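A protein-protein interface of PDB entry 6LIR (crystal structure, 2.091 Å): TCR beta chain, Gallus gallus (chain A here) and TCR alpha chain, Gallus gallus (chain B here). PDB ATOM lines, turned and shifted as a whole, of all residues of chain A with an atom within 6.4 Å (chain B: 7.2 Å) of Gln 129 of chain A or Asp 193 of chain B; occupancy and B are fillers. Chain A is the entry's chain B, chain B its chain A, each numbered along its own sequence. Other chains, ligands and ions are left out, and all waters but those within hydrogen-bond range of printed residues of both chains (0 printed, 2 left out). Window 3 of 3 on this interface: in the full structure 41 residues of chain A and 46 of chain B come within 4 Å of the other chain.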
ATOM      1  N   PRO A 126     -16.210 -10.393 -21.296  1.00  0.00           N
ATOM      2  CA  PRO A 126     -15.184  -9.890 -22.210  1.00  0.00           C
ATOM      3  C   PRO A 126     -15.671  -9.940 -23.648  1.00  0.00           C
ATOM      4  O   PRO A 126     -16.536 -10.741 -24.013  1.00  0.00           O
ATOM      5  CB  PRO A 126     -14.008 -10.844 -21.987  1.00  0.00           C
ATOM      6  CG  PRO A 126     -14.644 -12.106 -21.522  1.00  0.00           C
ATOM      7  CD  PRO A 126     -15.843 -11.694 -20.711  1.00  0.00           C
ATOM      8  N   SER A 127     -15.117  -9.049 -24.463  1.00  0.00           N
ATOM      9  CA  SER A 127     -15.554  -8.934 -25.847  1.00  0.00           C
ATOM     10  C   SER A 127     -15.059 -10.120 -26.662  1.00  0.00           C
ATOM     11  O   SER A 127     -13.866 -10.439 -26.657  1.00  0.00           O
ATOM     12  CB  SER A 127     -15.037  -7.628 -26.450  1.00  0.00           C
ATOM     13  OG  SER A 127     -15.346  -7.547 -27.830  1.00  0.00           O
ATOM     14  N   LYS A 128     -15.981 -10.765 -27.382  1.00  0.00           N
ATOM     15  CA  LYS A 128     -15.586 -11.845 -28.281  1.00  0.00           C
ATOM     16  C   LYS A 128     -14.714 -11.320 -29.412  1.00  0.00           C
ATOM     17  O   LYS A 128     -13.830 -12.033 -29.901  1.00  0.00           O
ATOM     18  CB  LYS A 128     -16.824 -12.557 -28.835  1.00  0.00           C
ATOM     19  CG  LYS A 128     -17.749 -13.114 -27.762  1.00  0.00           C
ATOM     20  CD  LYS A 128     -18.431 -14.402 -28.218  1.00  0.00           C
ATOM     21  CE  LYS A 128     -19.185 -15.064 -27.069  1.00  0.00           C
ATOM     22  NZ  LYS A 128     -18.643 -16.412 -26.723  1.00  0.00           N
ATOM     23  N   GLN A 129     -14.929 -10.068 -29.819  1.00  0.00           N
ATOM     24  CA  GLN A 129     -14.102  -9.472 -30.862  1.00  0.00           C
ATOM     25  C   GLN A 129     -12.676  -9.241 -30.373  1.00  0.00           C
ATOM     26  O   GLN A 129     -11.717  -9.508 -31.107  1.00  0.00           O
ATOM     27  CB  GLN A 129     -14.726  -8.169 -31.355  1.00  0.00           C
ATOM     28  CG  GLN A 129     -14.085  -7.635 -32.621  1.00  0.00           C
ATOM     29  CD  GLN A 129     -14.550  -6.239 -32.963  1.00  0.00           C
ATOM     30  OE1 GLN A 129     -15.555  -5.762 -32.433  1.00  0.00           O
ATOM     31  NE2 GLN A 129     -13.818  -5.568 -33.848  1.00  0.00           N
ATOM     32  N   GLU A 130     -12.510  -8.710 -29.154  1.00  0.00           N
ATOM     33  CA  GLU A 130     -11.167  -8.568 -28.596  1.00  0.00           C
ATOM     34  C   GLU A 130     -10.454  -9.914 -28.552  1.00  0.00           C
ATOM     35  O   GLU A 130      -9.291 -10.030 -28.955  1.00  0.00           O
ATOM     36  CB  GLU A 130     -11.217  -7.953 -27.192  1.00  0.00           C
ATOM     37  CG  GLU A 130      -9.858  -7.996 -26.469  1.00  0.00           C
ATOM     38  CD  GLU A 130      -9.926  -7.624 -24.983  1.00  0.00           C
ATOM     39  OE1 GLU A 130      -8.948  -7.033 -24.475  1.00  0.00           O
ATOM     40  OE2 GLU A 130     -10.945  -7.919 -24.323  1.00  0.00           O
ATOM     41  N   ILE A 131     -11.147 -10.945 -28.062  1.00  0.00           N
ATOM     42  CA  ILE A 131     -10.562 -12.282 -27.970  1.00  0.00           C
ATOM     43  C   ILE A 131     -10.048 -12.739 -29.331  1.00  0.00           C
ATOM     44  O   ILE A 131      -8.942 -13.276 -29.449  1.00  0.00           O
ATOM     45  CB  ILE A 131     -11.592 -13.275 -27.398  1.00  0.00           C
ATOM     46  CG1 ILE A 131     -11.944 -12.907 -25.955  1.00  0.00           C
ATOM     47  CG2 ILE A 131     -11.064 -14.693 -27.469  1.00  0.00           C
ATOM     48  CD1 ILE A 131     -13.147 -13.659 -25.410  1.00  0.00           C
ATOM     49  N   GLN A 132     -10.861 -12.568 -30.373  1.00  0.00           N
ATOM     50  CA  GLN A 132     -10.430 -12.963 -31.712  1.00  0.00           C
ATOM     51  C   GLN A 132      -9.291 -12.083 -32.220  1.00  0.00           C
ATOM     52  O   GLN A 132      -8.289 -12.590 -32.741  1.00  0.00           O
ATOM     53  CB  GLN A 132     -11.614 -12.936 -32.676  1.00  0.00           C
ATOM     54  CG  GLN A 132     -12.622 -14.034 -32.382  1.00  0.00           C
ATOM     55  CD  GLN A 132     -13.949 -13.840 -33.087  1.00  0.00           C
ATOM     56  OE1 GLN A 132     -15.006 -13.888 -32.459  1.00  0.00           O
ATOM     57  NE2 GLN A 132     -13.904 -13.640 -34.401  1.00  0.00           N
ATOM     58  N   GLU A 133      -9.441 -10.758 -32.117  1.00  0.00           N
ATOM     59  CA  GLU A 133      -8.441  -9.850 -32.684  1.00  0.00           C
ATOM     60  C   GLU A 133      -7.123  -9.897 -31.916  1.00  0.00           C
ATOM     61  O   GLU A 133      -6.044  -9.924 -32.522  1.00  0.00           O
ATOM     62  CB  GLU A 133      -8.983  -8.422 -32.715  1.00  0.00           C
ATOM     63  CG  GLU A 133     -10.129  -8.213 -33.685  1.00  0.00           C
ATOM     64  CD  GLU A 133     -10.712  -6.817 -33.597  1.00  0.00           C
ATOM     65  OE1 GLU A 133     -10.217  -6.020 -32.772  1.00  0.00           O
ATOM     66  OE2 GLU A 133     -11.661  -6.515 -34.353  1.00  0.00           O
ATOM     67  N   LYS A 134      -7.185  -9.871 -30.579  1.00  0.00           N
ATOM     68  CA  LYS A 134      -5.989  -9.732 -29.754  1.00  0.00           C
ATOM     69  C   LYS A 134      -5.549 -11.015 -29.064  1.00  0.00           C
ATOM     70  O   LYS A 134      -4.495 -11.014 -28.416  1.00  0.00           O
ATOM     71  CB  LYS A 134      -6.209  -8.659 -28.676  1.00  0.00           C
ATOM     72  CG  LYS A 134      -6.813  -7.364 -29.183  1.00  0.00           C
ATOM     73  CD  LYS A 134      -5.850  -6.625 -30.088  1.00  0.00           C
ATOM     74  CE  LYS A 134      -6.382  -5.243 -30.423  1.00  0.00           C
ATOM     75  NZ  LYS A 134      -5.399  -4.427 -31.185  1.00  0.00           N
ATOM     76  N   LYS A 135      -6.322 -12.099 -29.172  1.00  0.00           N
ATOM     77  CA  LYS A 135      -6.037 -13.348 -28.457  1.00  0.00           C
ATOM     78  C   LYS A 135      -5.902 -13.113 -26.953  1.00  0.00           C
ATOM     79  O   LYS A 135      -5.177 -13.827 -26.257  1.00  0.00           O
ATOM     80  CB  LYS A 135      -4.800 -14.051 -29.025  1.00  0.00           C
ATOM     81  CG  LYS A 135      -5.134 -14.938 -30.229  1.00  0.00           C
ATOM     82  CD  LYS A 135      -3.926 -15.708 -30.747  1.00  0.00           C
ATOM     83  CE  LYS A 135      -3.378 -16.671 -29.703  1.00  0.00           C
ATOM     84  NZ  LYS A 135      -3.128 -18.030 -30.271  1.00  0.00           N
ATOM     85  N   SER B 116      -7.831  -0.395 -30.391  1.00  0.00           N
ATOM     86  CA  SER B 116      -9.135  -0.985 -30.641  1.00  0.00           C
ATOM     87  C   SER B 116     -10.082  -0.544 -29.540  1.00  0.00           C
ATOM     88  O   SER B 116      -9.665  -0.255 -28.415  1.00  0.00           O
ATOM     89  CB  SER B 116      -9.076  -2.512 -30.690  1.00  0.00           C
ATOM     90  OG  SER B 116      -8.132  -2.951 -31.643  1.00  0.00           O
ATOM     91  N   VAL B 117     -11.356  -0.459 -29.892  1.00  0.00           N
ATOM     92  CA  VAL B 117     -12.405  -0.040 -28.979  1.00  0.00           C
ATOM     93  C   VAL B 117     -13.478  -1.120 -28.977  1.00  0.00           C
ATOM     94  O   VAL B 117     -13.787  -1.697 -30.025  1.00  0.00           O
ATOM     95  CB  VAL B 117     -12.964   1.344 -29.373  1.00  0.00           C
ATOM     96  CG1 VAL B 117     -14.170   1.682 -28.559  1.00  0.00           C
ATOM     97  CG2 VAL B 117     -11.902   2.413 -29.156  1.00  0.00           C
ATOM     98  N   TYR B 118     -14.049  -1.397 -27.804  1.00  0.00           N
ATOM     99  CA  TYR B 118     -15.043  -2.452 -27.680  1.00  0.00           C
ATOM    100  C   TYR B 118     -16.099  -2.046 -26.667  1.00  0.00           C
ATOM    101  O   TYR B 118     -15.826  -1.323 -25.707  1.00  0.00           O
ATOM    102  CB  TYR B 118     -14.435  -3.788 -27.221  1.00  0.00           C
ATOM    103  CG  TYR B 118     -13.217  -4.250 -27.983  1.00  0.00           C
ATOM    104  CD1 TYR B 118     -13.340  -4.906 -29.201  1.00  0.00           C
ATOM    105  CD2 TYR B 118     -11.943  -4.042 -27.476  1.00  0.00           C
ATOM    106  CE1 TYR B 118     -12.224  -5.337 -29.894  1.00  0.00           C
ATOM    107  CE2 TYR B 118     -10.824  -4.466 -28.161  1.00  0.00           C
ATOM    108  CZ  TYR B 118     -10.968  -5.112 -29.367  1.00  0.00           C
ATOM    109  OH  TYR B 118      -9.850  -5.534 -30.049  1.00  0.00           O
ATOM    110  N   ARG B 119     -17.304  -2.559 -26.878  1.00  0.00           N
ATOM    111  CA  ARG B 119     -18.408  -2.383 -25.952  1.00  0.00           C
ATOM    112  C   ARG B 119     -18.611  -3.682 -25.193  1.00  0.00           C
ATOM    113  O   ARG B 119     -18.586  -4.767 -25.783  1.00  0.00           O
ATOM    114  CB  ARG B 119     -19.697  -2.010 -26.682  1.00  0.00           C
ATOM    115  CG  ARG B 119     -19.933  -0.525 -26.813  1.00  0.00           C
ATOM    116  CD  ARG B 119     -20.325  -0.171 -28.233  1.00  0.00           C
ATOM    117  NE  ARG B 119     -21.552  -0.843 -28.657  1.00  0.00           N
ATOM    118  CZ  ARG B 119     -22.773  -0.339 -28.500  1.00  0.00           C
ATOM    119  NH1 ARG B 119     -22.935   0.845 -27.923  1.00  0.00           N
ATOM    120  NH2 ARG B 119     -23.834  -1.019 -28.918  1.00  0.00           N
ATOM    121  N   LEU B 120     -18.829  -3.571 -23.891  1.00  0.00           N
ATOM    122  CA  LEU B 120     -19.019  -4.739 -23.054  1.00  0.00           C
ATOM    123  C   LEU B 120     -20.334  -4.621 -22.308  1.00  0.00           C
ATOM    124  O   LEU B 120     -20.788  -3.522 -21.975  1.00  0.00           O
ATOM    125  CB  LEU B 120     -17.886  -4.899 -22.033  1.00  0.00           C
ATOM    126  CG  LEU B 120     -16.443  -4.693 -22.488  1.00  0.00           C
ATOM    127  CD1 LEU B 120     -15.492  -4.936 -21.321  1.00  0.00           C
ATOM    128  CD2 LEU B 120     -16.119  -5.609 -23.646  1.00  0.00           C
ATOM    129  N   CYS B 180     -19.413   4.538 -27.433  1.00  0.00           N
ATOM    130  CA  CYS B 180     -18.066   4.018 -27.246  1.00  0.00           C
ATOM    131  C   CYS B 180     -17.242   4.404 -28.459  1.00  0.00           C
ATOM    132  O   CYS B 180     -17.465   3.883 -29.555  1.00  0.00           O
ATOM    133  CB  CYS B 180     -18.154   2.501 -27.125  1.00  0.00           C
ATOM    134  SG  CYS B 180     -16.779   1.562 -26.507  1.00  0.00           S
ATOM    135  N   LYS B 191     -14.697   3.188 -33.259  1.00  0.00           N
ATOM    136  CA  LYS B 191     -16.064   3.042 -32.781  1.00  0.00           C
ATOM    137  C   LYS B 191     -16.292   1.580 -32.430  1.00  0.00           C
ATOM    138  O   LYS B 191     -15.696   0.689 -33.040  1.00  0.00           O
ATOM    139  CB  LYS B 191     -17.088   3.531 -33.817  1.00  0.00           C
ATOM    140  CG  LYS B 191     -17.325   5.038 -33.770  1.00  0.00           C
ATOM    141  CD  LYS B 191     -17.741   5.596 -35.123  1.00  0.00           C
ATOM    142  CE  LYS B 191     -19.022   4.953 -35.604  1.00  0.00           C
ATOM    143  NZ  LYS B 191     -19.486   5.472 -36.919  1.00  0.00           N
ATOM    144  N   GLY B 192     -17.100   1.335 -31.404  1.00  0.00           N
ATOM    145  CA  GLY B 192     -17.384  -0.020 -30.963  1.00  0.00           C
ATOM    146  C   GLY B 192     -18.730  -0.521 -31.465  1.00  0.00           C
ATOM    147  O   GLY B 192     -19.687   0.243 -31.585  1.00  0.00           O
ATOM    148  N   ASP B 193     -18.773  -1.815 -31.764  1.00  0.00           N
ATOM    149  CA  ASP B 193     -19.965  -2.577 -32.125  1.00  0.00           C
ATOM    150  C   ASP B 193     -20.121  -3.713 -31.112  1.00  0.00           C
ATOM    151  O   ASP B 193     -19.400  -3.779 -30.111  1.00  0.00           O
ATOM    152  CB  ASP B 193     -19.902  -3.081 -33.573  1.00  0.00           C
ATOM    153  CG  ASP B 193     -18.619  -3.813 -33.887  1.00  0.00           C
ATOM    154  OD1 ASP B 193     -17.731  -3.855 -33.010  1.00  0.00           O
ATOM    155  OD2 ASP B 193     -18.498  -4.347 -35.012  1.00  0.00           O
ATOM    156  N   ASP B 194     -21.083  -4.594 -31.350  1.00  0.00           N
ATOM    157  CA  ASP B 194     -21.448  -5.642 -30.408  1.00  0.00           C
ATOM    158  C   ASP B 194     -21.594  -6.968 -31.136  1.00  0.00           C
ATOM    159  O   ASP B 194     -21.501  -7.019 -32.367  1.00  0.00           O
ATOM    160  CB  ASP B 194     -22.757  -5.241 -29.706  1.00  0.00           C
ATOM    161  CG  ASP B 194     -22.516  -4.607 -28.358  1.00  0.00           C
ATOM    162  OD1 ASP B 194     -21.967  -5.289 -27.465  1.00  0.00           O
ATOM    163  OD2 ASP B 194     -22.870  -3.421 -28.194  1.00  0.00           O
ATOM    164  N   PRO B 195     -21.820  -8.085 -30.402  1.00  0.00           N
ATOM    165  CA  PRO B 195     -21.730  -9.393 -31.072  1.00  0.00           C
ATOM    166  C   PRO B 195     -22.723  -9.614 -32.208  1.00  0.00           C
ATOM    167  O   PRO B 195     -22.424 -10.442 -33.071  1.00  0.00           O
ATOM    168  CB  PRO B 195     -22.008 -10.391 -29.933  1.00  0.00           C
ATOM    169  CG  PRO B 195     -22.622  -9.583 -28.837  1.00  0.00           C
ATOM    170  CD  PRO B 195     -21.961  -8.255 -28.943  1.00  0.00           C
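The side-chain hydroxyl (OH) of Tyr 118 of chain B lies within hydrogen-bond range of the side-chain carboxylate (OE1) of Glu 133 of chain A.
The side-chain carboxylate of Asp 193 of chain B sits close to the side-chain amide oxygen of Gln 129 of chain A.
The side-chain hydroxyl of Ser 116 of chain B lies close to the side-chain amino group of Lys 134 of chain A (3.1 Å).
OG of Ser 116 of chain B lies close to OH of Tyr 118 of chain B, 3.5 Å away.
N of Glu 130 of chain A is in hydrogen-bond range of OG of Ser 127 of chain A (3.3 Å).
The backbone NH (N) of Gln 129 of chain A sits close to the side-chain hydroxyl (OG) of Ser 127 of chain A, at 3.2 Å.
The side-chain carboxylate (OE2) of Glu 133 of chain A is in hydrogen-bond range of the side-chain amide nitrogen (NE2) of Gln 129 of chain A, at 2.4 Å.
Of the 11 printed residues of chain B, 4 touch a printed residue of chain A.
Printed residues of chain B that touch a printed residue of chain A: Ser 116, Tyr 118, Leu 120 and Asp 193.
Hydrophobic or aromatic side chains of chain B that line the printed part of chain A: Tyr 118 and Leu 120.
Printed residues of chain A that touch a printed residue of chain B: Ser 127, Gln 129, Glu 130, Glu 133 and Lys 134.
Among the printed residues, no Asp or Glu carboxylate lies within 4 Å of a Lys or Arg side-chain nitrogen of the other chain.
Gln 129 of chain A touches just these residues of chain B: Tyr 118 (3.96 Å) and Asp 193 (3.0 Å).
Printed residues of chain A within 4 Å of Asp 193 of chain B: Gln 129 (3.0 Å).
Printed residues of chain B within 4 Å of Glu 130 of chain A: Tyr 118 (3.5 Å).
Printed residues of chain B within 4 Å of Lys 134 of chain A: Ser 116 and Tyr 118.
Printed residues of chain A within 4 Å of Ser 116 of chain B: Glu 133 and Lys 134.
Printed residues of chain B within 4 Å of Ser 127 of chain A: Tyr 118 and Leu 120.
Arg 119 of chain B touches none of the printed residues of chain A.
The nearest printed residue of chain B that does not touch Glu 133 of chain A is Val 117 of chain B (6.2 Å).
CD1 of Tyr 118 of chain B touches OG of Ser 127 of chain A, 3.6 Å away.
Leu 120 of chain B touches Ser 127 of chain A (CD2 to CB, 3.6 Å).
Gln 129 of chain A touches Tyr 118 of chain B.
CE1 of Tyr 118 of chain B touches N of Glu 130 of chain A (3.5 Å).
OE1 of Glu 133 of chain A touches OG of Ser 116 of chain B, at 3.9 Å.
Tyr 118 of chain B touches Lys 134 of chain A.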
